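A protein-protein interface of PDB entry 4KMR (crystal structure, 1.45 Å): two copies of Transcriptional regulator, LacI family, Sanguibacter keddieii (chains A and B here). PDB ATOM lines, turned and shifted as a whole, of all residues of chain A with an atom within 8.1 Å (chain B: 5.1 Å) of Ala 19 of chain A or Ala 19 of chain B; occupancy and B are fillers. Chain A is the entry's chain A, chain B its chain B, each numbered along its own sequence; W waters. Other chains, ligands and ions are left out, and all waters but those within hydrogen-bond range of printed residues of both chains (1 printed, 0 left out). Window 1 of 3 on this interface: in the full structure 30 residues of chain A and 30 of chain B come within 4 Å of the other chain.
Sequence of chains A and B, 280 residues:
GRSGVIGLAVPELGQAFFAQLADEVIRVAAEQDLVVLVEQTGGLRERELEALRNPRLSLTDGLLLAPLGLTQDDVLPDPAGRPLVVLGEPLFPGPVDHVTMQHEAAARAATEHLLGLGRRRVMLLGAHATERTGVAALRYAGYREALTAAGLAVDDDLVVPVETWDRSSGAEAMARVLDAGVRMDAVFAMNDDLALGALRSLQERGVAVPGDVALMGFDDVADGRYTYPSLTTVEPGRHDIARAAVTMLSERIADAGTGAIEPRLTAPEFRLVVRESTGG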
ATOM      1  N   LEU A   8       9.978  12.166 -13.528  1.00  0.00           N
ATOM      2  CA  LEU A   8      10.644  11.658 -14.696  1.00  0.00           C
ATOM      3  C   LEU A   8      10.041  12.431 -15.887  1.00  0.00           C
ATOM      4  O   LEU A   8       8.834  12.278 -16.184  1.00  0.00           O
ATOM      5  CB  LEU A   8      10.394  10.170 -14.893  1.00  0.00           C
ATOM      6  CG  LEU A   8      10.893   9.547 -16.186  1.00  0.00           C
ATOM      7  CD1 LEU A   8      12.403   9.704 -16.333  1.00  0.00           C
ATOM      8  CD2 LEU A   8      10.536   8.078 -16.271  1.00  0.00           C
ATOM      9  N   VAL A  10      10.273  12.954 -19.822  1.00  0.00           N
ATOM     10  CA  VAL A  10      10.706  12.323 -21.052  1.00  0.00           C
ATOM     11  C   VAL A  10       9.948  12.993 -22.212  1.00  0.00           C
ATOM     12  O   VAL A  10       8.882  13.601 -22.016  1.00  0.00           O
ATOM     13  CB  VAL A  10      10.404  10.815 -21.062  1.00  0.00           C
ATOM     14  CG1 VAL A  10      11.209  10.070 -20.004  1.00  0.00           C
ATOM     15  CG2 VAL A  10       8.925  10.555 -20.859  1.00  0.00           C
ATOM     16  N   GLU A  12       8.028  11.649 -24.712  1.00  0.00           N
ATOM     17  CA  GLU A  12       6.687  11.047 -24.816  1.00  0.00           C
ATOM     18  C   GLU A  12       6.772   9.549 -24.514  1.00  0.00           C
ATOM     19  O   GLU A  12       7.797   8.920 -24.855  1.00  0.00           O
ATOM     20  CB  GLU A  12       6.109  11.191 -26.202  1.00  0.00           C
ATOM     21  CG  GLU A  12       7.013  10.700 -27.297  1.00  0.00           C
ATOM     22  CD  GLU A  12       6.315  10.721 -28.659  1.00  0.00           C
ATOM     23  OE1 GLU A  12       6.904  11.203 -29.648  1.00  0.00           O
ATOM     24  OE2 GLU A  12       5.146  10.288 -28.717  1.00  0.00           O
ATOM     25  N   LEU A  13       5.736   8.990 -23.861  1.00  0.00           N
ATOM     26  CA  LEU A  13       5.664   7.539 -23.620  1.00  0.00           C
ATOM     27  C   LEU A  13       5.317   6.684 -24.822  1.00  0.00           C
ATOM     28  O   LEU A  13       5.531   5.448 -24.815  1.00  0.00           O
ATOM     29  CB  LEU A  13       4.697   7.209 -22.477  1.00  0.00           C
ATOM     30  CG  LEU A  13       5.097   7.742 -21.096  1.00  0.00           C
ATOM     31  CD1 LEU A  13       4.016   7.393 -20.079  1.00  0.00           C
ATOM     32  CD2 LEU A  13       6.421   7.204 -20.611  1.00  0.00           C
ATOM     33  N   GLY A  14       4.809   7.313 -25.856  1.00  0.00           N
ATOM     34  CA  GLY A  14       4.494   6.621 -27.121  1.00  0.00           C
ATOM     35  C   GLY A  14       5.785   6.149 -27.798  1.00  0.00           C
ATOM     36  O   GLY A  14       5.747   5.377 -28.782  1.00  0.00           O
ATOM     37  N   GLN A  15       6.932   6.670 -27.340  1.00  0.00           N
ATOM     38  CA  GLN A  15       8.245   6.226 -27.840  1.00  0.00           C
ATOM     39  C   GLN A  15       8.685   5.019 -26.979  1.00  0.00           C
ATOM     40  O   GLN A  15       8.824   5.142 -25.761  1.00  0.00           O
ATOM     41  CB  GLN A  15       9.297   7.361 -27.793  1.00  0.00           C
ATOM     42  CG  GLN A  15       9.127   8.446 -28.843  1.00  0.00           C
ATOM     43  CD  GLN A  15      10.191   9.540 -28.740  1.00  0.00           C
ATOM     44  OE1 GLN A  15      11.356   9.252 -28.491  1.00  0.00           O
ATOM     45  NE2 GLN A  15       9.800  10.787 -28.983  1.00  0.00           N
ATOM     46  N   ALA A  16       8.822   3.851 -27.608  1.00  0.00           N
ATOM     47  CA  ALA A  16       9.123   2.627 -26.855  1.00  0.00           C
ATOM     48  C   ALA A  16      10.335   2.753 -25.955  1.00  0.00           C
ATOM     49  O   ALA A  16      10.342   2.213 -24.839  1.00  0.00           O
ATOM     50  CB  ALA A  16       9.257   1.440 -27.778  1.00  0.00           C
ATOM     51  N   PHE A  17      11.385   3.413 -26.413  1.00  0.00           N
ATOM     52  CA  PHE A  17      12.546   3.557 -25.561  1.00  0.00           C
ATOM     53  C   PHE A  17      12.206   4.211 -24.218  1.00  0.00           C
ATOM     54  O   PHE A  17      12.659   3.764 -23.137  1.00  0.00           O
ATOM     55  CB  PHE A  17      13.612   4.387 -26.250  1.00  0.00           C
ATOM     56  CG  PHE A  17      14.820   4.569 -25.414  1.00  0.00           C
ATOM     57  CD1 PHE A  17      15.842   3.645 -25.435  1.00  0.00           C
ATOM     58  CD2 PHE A  17      14.927   5.658 -24.578  1.00  0.00           C
ATOM     59  CE1 PHE A  17      16.962   3.825 -24.627  1.00  0.00           C
ATOM     60  CE2 PHE A  17      16.021   5.824 -23.766  1.00  0.00           C
ATOM     61  CZ  PHE A  17      17.033   4.899 -23.769  1.00  0.00           C
ATOM     62  N   PHE A  18      11.437   5.304 -24.267  1.00  0.00           N
ATOM     63  CA  PHE A  18      11.093   6.011 -23.048  1.00  0.00           C
ATOM     64  C   PHE A  18      10.071   5.282 -22.209  1.00  0.00           C
ATOM     65  O   PHE A  18      10.133   5.373 -20.989  1.00  0.00           O
ATOM     66  CB  PHE A  18      10.715   7.456 -23.352  1.00  0.00           C
ATOM     67  CG  PHE A  18      11.900   8.255 -23.850  1.00  0.00           C
ATOM     68  CD1 PHE A  18      12.954   8.516 -23.020  1.00  0.00           C
ATOM     69  CD2 PHE A  18      11.985   8.662 -25.157  1.00  0.00           C
ATOM     70  CE1 PHE A  18      14.067   9.228 -23.454  1.00  0.00           C
ATOM     71  CE2 PHE A  18      13.086   9.356 -25.614  1.00  0.00           C
ATOM     72  CZ  PHE A  18      14.139   9.646 -24.752  1.00  0.00           C
ATOM     73  N   ALA A  19       9.127   4.572 -22.842  1.00  0.00           N
ATOM     74  CA  ALA A  19       8.157   3.797 -22.083  1.00  0.00           C
ATOM     75  C   ALA A  19       8.899   2.703 -21.292  1.00  0.00           C
ATOM     76  O   ALA A  19       8.571   2.438 -20.139  1.00  0.00           O
ATOM     77  CB  ALA A  19       7.155   3.171 -22.993  1.00  0.00           C
ATOM     78  N   GLN A  20       9.847   2.024 -21.957  1.00  0.00           N
ATOM     79  CA  GLN A  20      10.593   0.953 -21.290  1.00  0.00           C
ATOM     80  C   GLN A  20      11.541   1.471 -20.224  1.00  0.00           C
ATOM     81  O   GLN A  20      11.709   0.846 -19.174  1.00  0.00           O
ATOM     82  CB  GLN A  20      11.258   0.062 -22.349  1.00  0.00           C
ATOM     83  CG  GLN A  20      10.181  -0.671 -23.132  1.00  0.00           C
ATOM     84  CD  GLN A  20      10.743  -1.590 -24.199  1.00  0.00           C
ATOM     85  OE1 GLN A  20      11.882  -2.048 -24.093  1.00  0.00           O
ATOM     86  NE2 GLN A  20       9.951  -1.865 -25.227  1.00  0.00           N
ATOM     87  N   LEU A  21      12.142   2.611 -20.462  1.00  0.00           N
ATOM     88  CA  LEU A  21      12.983   3.240 -19.448  1.00  0.00           C
ATOM     89  C   LEU A  21      12.127   3.632 -18.212  1.00  0.00           C
ATOM     90  O   LEU A  21      12.511   3.419 -17.075  1.00  0.00           O
ATOM     91  CB  LEU A  21      13.658   4.470 -20.020  1.00  0.00           C
ATOM     92  CG  LEU A  21      14.568   5.191 -19.028  1.00  0.00           C
ATOM     93  CD1 LEU A  21      15.631   4.237 -18.494  1.00  0.00           C
ATOM     94  CD2 LEU A  21      15.223   6.364 -19.734  1.00  0.00           C
ATOM     95  N   ALA A  22      10.966   4.232 -18.463  1.00  0.00           N
ATOM     96  CA  ALA A  22      10.035   4.577 -17.404  1.00  0.00           C
ATOM     97  C   ALA A  22       9.632   3.355 -16.577  1.00  0.00           C
ATOM     98  O   ALA A  22       9.555   3.436 -15.348  1.00  0.00           O
ATOM     99  CB  ALA A  22       8.803   5.309 -17.946  1.00  0.00           C
ATOM    100  N   ASP A  23       9.304   2.244 -17.244  1.00  0.00           N
ATOM    101  CA  ASP A  23       8.937   1.002 -16.539  1.00  0.00           C
ATOM    102  C   ASP A  23      10.079   0.642 -15.571  1.00  0.00           C
ATOM    103  O   ASP A  23       9.845   0.334 -14.397  1.00  0.00           O
ATOM    104  CB  ASP A  23       8.751  -0.045 -17.633  1.00  0.00           C
ATOM    105  CG  ASP A  23       8.399  -1.410 -17.178  1.00  0.00           C
ATOM    106  OD1 ASP A  23       8.547  -1.811 -15.987  1.00  0.00           O
ATOM    107  OD2 ASP A  23       7.950  -2.149 -18.095  1.00  0.00           O
ATOM    108  N   GLU A  24      11.337   0.701 -16.065  1.00  0.00           N
ATOM    109  CA  GLU A  24      12.503   0.345 -15.204  1.00  0.00           C
ATOM    110  C   GLU A  24      12.679   1.353 -14.013  1.00  0.00           C
ATOM    111  O   GLU A  24      12.947   0.937 -12.899  1.00  0.00           O
ATOM    112  CB  GLU A  24      13.803   0.226 -15.990  1.00  0.00           C
ATOM    113  CG  GLU A  24      13.767  -0.801 -17.086  1.00  0.00           C
ATOM    114  CD  GLU A  24      13.597  -2.260 -16.635  1.00  0.00           C
ATOM    115  OE1 GLU A  24      13.443  -3.110 -17.565  1.00  0.00           O
ATOM    116  OE2 GLU A  24      13.648  -2.603 -15.410  1.00  0.00           O
ATOM    117  N   VAL A  25      12.542   2.650 -14.288  1.00  0.00           N
ATOM    118  CA  VAL A  25      12.619   3.686 -13.245  1.00  0.00           C
ATOM    119  C   VAL A  25      11.560   3.475 -12.183  1.00  0.00           C
ATOM    120  O   VAL A  25      11.843   3.544 -10.972  1.00  0.00           O
ATOM    121  CB  VAL A  25      12.525   5.077 -13.838  1.00  0.00           C
ATOM    122  CG1 VAL A  25      12.358   6.185 -12.782  1.00  0.00           C
ATOM    123  CG2 VAL A  25      13.783   5.376 -14.644  1.00  0.00           C
ATOM    124  N   ILE A  26      10.315   3.245 -12.610  1.00  0.00           N
ATOM    125  CA  ILE A  26       9.217   3.028 -11.653  1.00  0.00           C
ATOM    126  C   ILE A  26       9.524   1.823 -10.764  1.00  0.00           C
ATOM    127  O   ILE A  26       9.351   1.872  -9.539  1.00  0.00           O
ATOM    128  CB  ILE A  26       7.881   2.847 -12.396  1.00  0.00           C
ATOM    129  CG1 ILE A  26       7.523   4.206 -13.023  1.00  0.00           C
ATOM    130  CG2 ILE A  26       6.794   2.340 -11.447  1.00  0.00           C
ATOM    131  CD1 ILE A  26       6.430   4.097 -14.081  1.00  0.00           C
ATOM    132  N   VAL A  38       5.250  11.203 -13.927  1.00  0.00           N
ATOM    133  CA  VAL A  38       5.771  11.182 -15.296  1.00  0.00           C
ATOM    134  C   VAL A  38       5.205  12.401 -16.062  1.00  0.00           C
ATOM    135  O   VAL A  38       3.987  12.589 -16.132  1.00  0.00           O
ATOM    136  CB  VAL A  38       5.384   9.919 -16.037  1.00  0.00           C
ATOM    137  CG1 VAL A  38       5.898   9.953 -17.464  1.00  0.00           C
ATOM    138  CG2 VAL A  38       5.878   8.681 -15.278  1.00  0.00           C
ATOM    139  N   GLN A  40       5.657  14.722 -19.721  1.00  0.00           N
ATOM    140  CA  GLN A  40       6.065  14.626 -21.149  1.00  0.00           C
ATOM    141  C   GLN A  40       6.462  16.053 -21.576  1.00  0.00           C
ATOM    142  O   GLN A  40       5.758  17.038 -21.324  1.00  0.00           O
ATOM    143  CB  GLN A  40       4.958  14.074 -22.048  1.00  0.00           C
ATOM    144  CG  GLN A  40       4.691  12.606 -21.736  1.00  0.00           C
ATOM    145  CD  GLN A  40       3.580  11.928 -22.486  1.00  0.00           C
ATOM    146  OE1 GLN A  40       3.711  10.755 -22.808  1.00  0.00           O
ATOM    147  NE2 GLN A  40       2.476  12.607 -22.712  1.00  0.00           N
ATOM    148  N   VAL A 221      14.253  -2.390 -27.990  1.00  0.00           N
ATOM    149  CA  VAL A 221      12.931  -2.075 -27.458  1.00  0.00           C
ATOM    150  C   VAL A 221      11.783  -2.418 -28.387  1.00  0.00           C
ATOM    151  O   VAL A 221      10.638  -2.185 -28.018  1.00  0.00           O
ATOM    152  CB  VAL A 221      12.800  -0.604 -27.075  1.00  0.00           C
ATOM    153  CG1 VAL A 221      13.730  -0.260 -25.928  1.00  0.00           C
ATOM    154  CG2 VAL A 221      13.064   0.267 -28.275  1.00  0.00           C
ATOM    155  N   ARG A 238      19.551  -0.554 -20.105  1.00  0.00           N
ATOM    156  CA  ARG A 238      18.412   0.119 -19.425  1.00  0.00           C
ATOM    157  C   ARG A 238      18.256  -0.148 -17.951  1.00  0.00           C
ATOM    158  O   ARG A 238      17.940   0.768 -17.219  1.00  0.00           O
ATOM    159  CB  ARG A 238      17.046  -0.152 -20.090  1.00  0.00           C
ATOM    160  CG  ARG A 238      16.566   0.943 -21.037  1.00  0.00           C
ATOM    161  CD  ARG A 238      15.169   0.706 -21.622  1.00  0.00           C
ATOM    162  NE  ARG A 238      15.078  -0.585 -22.300  1.00  0.00           N
ATOM    163  CZ  ARG A 238      15.649  -0.880 -23.467  1.00  0.00           C
ATOM    164  NH1 ARG A 238      15.482  -2.104 -23.983  1.00  0.00           N
ATOM    165  NH2 ARG A 238      16.409   0.015 -24.107  1.00  0.00           N
ATOM    166  N   GLU B  12       1.712  -2.508 -17.373  1.00  0.00           N
ATOM    167  CA  GLU B  12       3.139  -2.109 -17.507  1.00  0.00           C
ATOM    168  C   GLU B  12       3.255  -1.189 -18.691  1.00  0.00           C
ATOM    169  O   GLU B  12       2.487  -1.276 -19.645  1.00  0.00           O
ATOM    170  CB  GLU B  12       4.080  -3.279 -17.707  1.00  0.00           C
ATOM    171  CG  GLU B  12       3.734  -4.098 -18.923  1.00  0.00           C
ATOM    172  CD  GLU B  12       4.664  -5.294 -19.204  1.00  0.00           C
ATOM    173  OE1 GLU B  12       5.900  -5.119 -19.189  1.00  0.00           O
ATOM    174  OE2 GLU B  12       4.157  -6.403 -19.514  1.00  0.00           O
ATOM    175  N   LEU B  13       4.203  -0.268 -18.627  1.00  0.00           N
ATOM    176  CA  LEU B  13       4.458   0.619 -19.737  1.00  0.00           C
ATOM    177  C   LEU B  13       5.175  -0.060 -20.917  1.00  0.00           C
ATOM    178  O   LEU B  13       5.179   0.483 -22.024  1.00  0.00           O
ATOM    179  CB  LEU B  13       5.214   1.869 -19.256  1.00  0.00           C
ATOM    180  CG  LEU B  13       4.440   2.775 -18.292  1.00  0.00           C
ATOM    181  CD1 LEU B  13       5.332   3.919 -17.765  1.00  0.00           C
ATOM    182  CD2 LEU B  13       3.181   3.414 -18.895  1.00  0.00           C
ATOM    183  N   GLY B  14       5.797  -1.217 -20.690  1.00  0.00           N
ATOM    184  CA  GLY B  14       6.427  -1.966 -21.769  1.00  0.00           C
ATOM    185  C   GLY B  14       5.418  -2.555 -22.765  1.00  0.00           C
ATOM    186  O   GLY B  14       5.834  -3.088 -23.802  1.00  0.00           O
ATOM    187  N   GLN B  15       4.112  -2.468 -22.461  1.00  0.00           N
ATOM    188  CA  GLN B  15       3.023  -2.926 -23.372  1.00  0.00           C
ATOM    189  C   GLN B  15       2.582  -1.718 -24.193  1.00  0.00           C
ATOM    190  O   GLN B  15       2.076  -0.742 -23.632  1.00  0.00           O
ATOM    191  CB  GLN B  15       1.845  -3.499 -22.606  1.00  0.00           C
ATOM    192  CG  GLN B  15       2.113  -4.861 -22.014  1.00  0.00           C
ATOM    193  CD  GLN B  15       0.913  -5.428 -21.248  1.00  0.00           C
ATOM    194  OE1 GLN B  15      -0.235  -5.234 -21.633  1.00  0.00           O
ATOM    195  NE2 GLN B  15       1.180  -6.098 -20.150  1.00  0.00           N
ATOM    196  N   ALA B  16       2.797  -1.789 -25.511  1.00  0.00           N
ATOM    197  CA  ALA B  16       2.534  -0.682 -26.395  1.00  0.00           C
ATOM    198  C   ALA B  16       1.151   0.006 -26.241  1.00  0.00           C
ATOM    199  O   ALA B  16       1.043   1.226 -26.211  1.00  0.00           O
ATOM    200  CB  ALA B  16       2.844  -1.086 -27.813  1.00  0.00           C
ATOM    201  N   PHE B  17       0.099  -0.787 -26.073  1.00  0.00           N
ATOM    202  CA  PHE B  17      -1.225  -0.203 -25.936  1.00  0.00           C
ATOM    203  C   PHE B  17      -1.278   0.691 -24.696  1.00  0.00           C
ATOM    204  O   PHE B  17      -1.852   1.803 -24.737  1.00  0.00           O
ATOM    205  CB  PHE B  17      -2.306  -1.239 -25.847  1.00  0.00           C
ATOM    206  CG  PHE B  17      -3.655  -0.670 -25.552  1.00  0.00           C
ATOM    207  CD1 PHE B  17      -4.373   0.014 -26.534  1.00  0.00           C
ATOM    208  CD2 PHE B  17      -4.158  -0.718 -24.269  1.00  0.00           C
ATOM    209  CE1 PHE B  17      -5.635   0.574 -26.245  1.00  0.00           C
ATOM    210  CE2 PHE B  17      -5.394  -0.141 -23.965  1.00  0.00           C
ATOM    211  CZ  PHE B  17      -6.135   0.507 -24.952  1.00  0.00           C
ATOM    212  N   PHE B  18      -0.732   0.197 -23.581  1.00  0.00           N
ATOM    213  CA  PHE B  18      -0.770   0.977 -22.344  1.00  0.00           C
ATOM    214  C   PHE B  18       0.147   2.159 -22.346  1.00  0.00           C
ATOM    215  O   PHE B  18      -0.176   3.180 -21.758  1.00  0.00           O
ATOM    216  CB  PHE B  18      -0.571   0.075 -21.135  1.00  0.00           C
ATOM    217  CG  PHE B  18      -1.750  -0.830 -20.914  1.00  0.00           C
ATOM    218  CD1 PHE B  18      -1.674  -2.166 -21.198  1.00  0.00           C
ATOM    219  CD2 PHE B  18      -2.968  -0.312 -20.497  1.00  0.00           C
ATOM    220  CE1 PHE B  18      -2.783  -2.986 -21.027  1.00  0.00           C
ATOM    221  CE2 PHE B  18      -4.066  -1.115 -20.372  1.00  0.00           C
ATOM    222  CZ  PHE B  18      -3.967  -2.450 -20.633  1.00  0.00           C
ATOM    223  N   ALA B  19       1.280   2.047 -23.009  1.00  0.00           N
ATOM    224  CA  ALA B  19       2.146   3.216 -23.118  1.00  0.00           C
ATOM    225  C   ALA B  19       1.448   4.341 -23.941  1.00  0.00           C
ATOM    226  O   ALA B  19       1.551   5.508 -23.609  1.00  0.00           O
ATOM    227  CB  ALA B  19       3.434   2.850 -23.799  1.00  0.00           C
ATOM    228  N   GLN B  20       0.791   3.958 -25.045  1.00  0.00           N
ATOM    229  CA  GLN B  20       0.070   4.910 -25.874  1.00  0.00           C
ATOM    230  C   GLN B  20      -1.094   5.535 -25.095  1.00  0.00           C
ATOM    231  O   GLN B  20      -1.321   6.748 -25.168  1.00  0.00           O
ATOM    232  CB  GLN B  20      -0.399   4.277 -27.201  1.00  0.00           C
ATOM    233  CG  GLN B  20       0.702   3.741 -28.093  1.00  0.00           C
ATOM    234  CD  GLN B  20       0.202   3.090 -29.403  1.00  0.00           C
ATOM    235  OE1 GLN B  20       1.012   2.684 -30.242  1.00  0.00           O
ATOM    236  NE2 GLN B  20      -1.124   3.002 -29.582  1.00  0.00           N
ATOM    237  N   LEU B  21      -1.821   4.716 -24.335  1.00  0.00           N
ATOM    238  CA  LEU B  21      -2.936   5.225 -23.542  1.00  0.00           C
ATOM    239  C   LEU B  21      -2.404   6.167 -22.418  1.00  0.00           C
ATOM    240  O   LEU B  21      -2.957   7.227 -22.182  1.00  0.00           O
ATOM    241  CB  LEU B  21      -3.720   4.057 -22.980  1.00  0.00           C
ATOM    242  CG  LEU B  21      -4.911   4.463 -22.127  1.00  0.00           C
ATOM    243  CD1 LEU B  21      -5.896   5.352 -22.882  1.00  0.00           C
ATOM    244  CD2 LEU B  21      -5.568   3.196 -21.592  1.00  0.00           C
ATOM    245  N   ALA B  22      -1.329   5.770 -21.744  1.00  0.00           N
ATOM    246  CA  ALA B  22      -0.707   6.586 -20.723  1.00  0.00           C
ATOM    247  C   ALA B  22      -0.282   7.942 -21.289  1.00  0.00           C
ATOM    248  O   ALA B  22      -0.465   8.973 -20.633  1.00  0.00           O
ATOM    249  CB  ALA B  22       0.428   5.870 -20.053  1.00  0.00           C
ATOM    250  N   ASP B  23       0.333   7.933 -22.473  1.00  0.00           N
ATOM    251  CA  ASP B  23       0.760   9.173 -23.130  1.00  0.00           C
ATOM    252  C   ASP B  23      -0.474  10.100 -23.297  1.00  0.00           C
ATOM    253  O   ASP B  23      -0.413  11.262 -22.933  1.00  0.00           O
ATOM    254  CB  ASP B  23       1.409   8.787 -24.455  1.00  0.00           C
ATOM    255  CG  ASP B  23       1.960   9.917 -25.238  1.00  0.00           C
ATOM    256  OD1 ASP B  23       2.961   9.611 -25.963  1.00  0.00           O
ATOM    257  OD2 ASP B  23       1.411  11.051 -25.217  1.00  0.00           O
HETATM  258  O   HOH W   1       7.319  -1.499 -25.557  1.00  0.00           O
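The backbone NH (N) of Gly 14 of chain A lies within hydrogen-bond range of the side-chain carboxylate (OD1) of Asp 23 of chain B (3.0 Å). OD2 of Asp 23 of chain B is in hydrogen-bond range of NE2 of Gln 40 of chain A, 3.1 Å away. The backbone NH of Gly 14 of chain B lies within hydrogen-bond range of the side-chain carboxylate of Asp 23 of chain A (3.5 Å).
N of Leu 13 of chain A is in hydrogen-bond range of OE1 of Gln 40 of chain A. OE2 of Glu 12 of chain B is in hydrogen-bond range of NE2 of Gln 15 of chain B. The side-chain carboxylate (OE1) of Glu 12 of chain A lies within hydrogen-bond range of the side-chain amide nitrogen (NE2) of Gln 15 of chain A (3.0 Å).
Among the printed residues, pairs that only touch across the chains: Ala 19 of chain A with Leu 13 of chain B, Leu 13 of chain A with Ala 19 of chain B, Glu 12 of chain A with Asp 23 of chain B, Leu 13 of chain A with Asp 23 of chain B, Ala 22 of chain A with Leu 13 of chain B, Asp 23 of chain A with Glu 12 of chain B, Ala 19 of chain A with Ala 19 of chain B, Ile 26 of chain A with Leu 13 of chain B and Leu 13 of chain A with Ala 22 of chain B.
Of the printed residues of chain B, Glu 12 of chain A touches Asp 23. Printed residues of chain B within 4 Å of Leu 13 of chain A: Ala 19 (3.5 Å), Ala 22 (3.9 Å) and Asp 23 (3.5 Å). Ala 19 of chain A touches just these residues of chain B: Leu 13 (3.5 Å) and Ala 19 (3.8 Å). Of the printed residues of chain B, Gln 40 of chain A touches Asp 23. Ala 19 of chain B touches two residues of chain A. Of the printed residues of chain A, Ala 22 of chain B touches Leu 13 (3.9 Å). Printed residues of chain A within 4 Å of Asp 23 of chain B: Glu 12 (3.5 Å), Leu 13 (3.5 Å), Gly 14 (3.0 Å) and Gln 40 (3.1 Å). The nearest residue of chain B that does not touch Ala 19 of chain A is Gly 14 of chain B (4.6 Å). The nearest residue of chain A that does not touch Ala 19 of chain B is Gly 14 of chain A (4.3 Å).
Hydrophobic or aromatic side chains of chain A that line the printed part of chain B: Leu 13, Ala 19, Ala 22 and Ile 26. Among the printed residues, no Asp or Glu carboxylate lies within 4 Å of a Lys or Arg side-chain nitrogen of the other chain.
Leu 13 of chain A touches Ala 19 of chain B, and with the chains exchanged Ala 19 of chain A touches Leu 13 of chain B. Leu 13 of chain A touches Asp 23 of chain B, but with the chains exchanged Asp 23 of chain A does not touch Leu 13 of chain B (4.2 Å). Gly 14 of chain A touches Asp 23 of chain B, and with the chains exchanged Asp 23 of chain A touches Gly 14 of chain B. Ala 19 of chain A touches its own counterpart, Ala 19 of chain B. Of the 12 pairs that touch across the chains among the printed residues, 9 have their exchanged pair printed and touching as well.
Water W1 lies within hydrogen-bond range of NE2 of Gln 20 of chain A (2.7 Å) and O of Gly 14 of chain B (2.8 Å).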
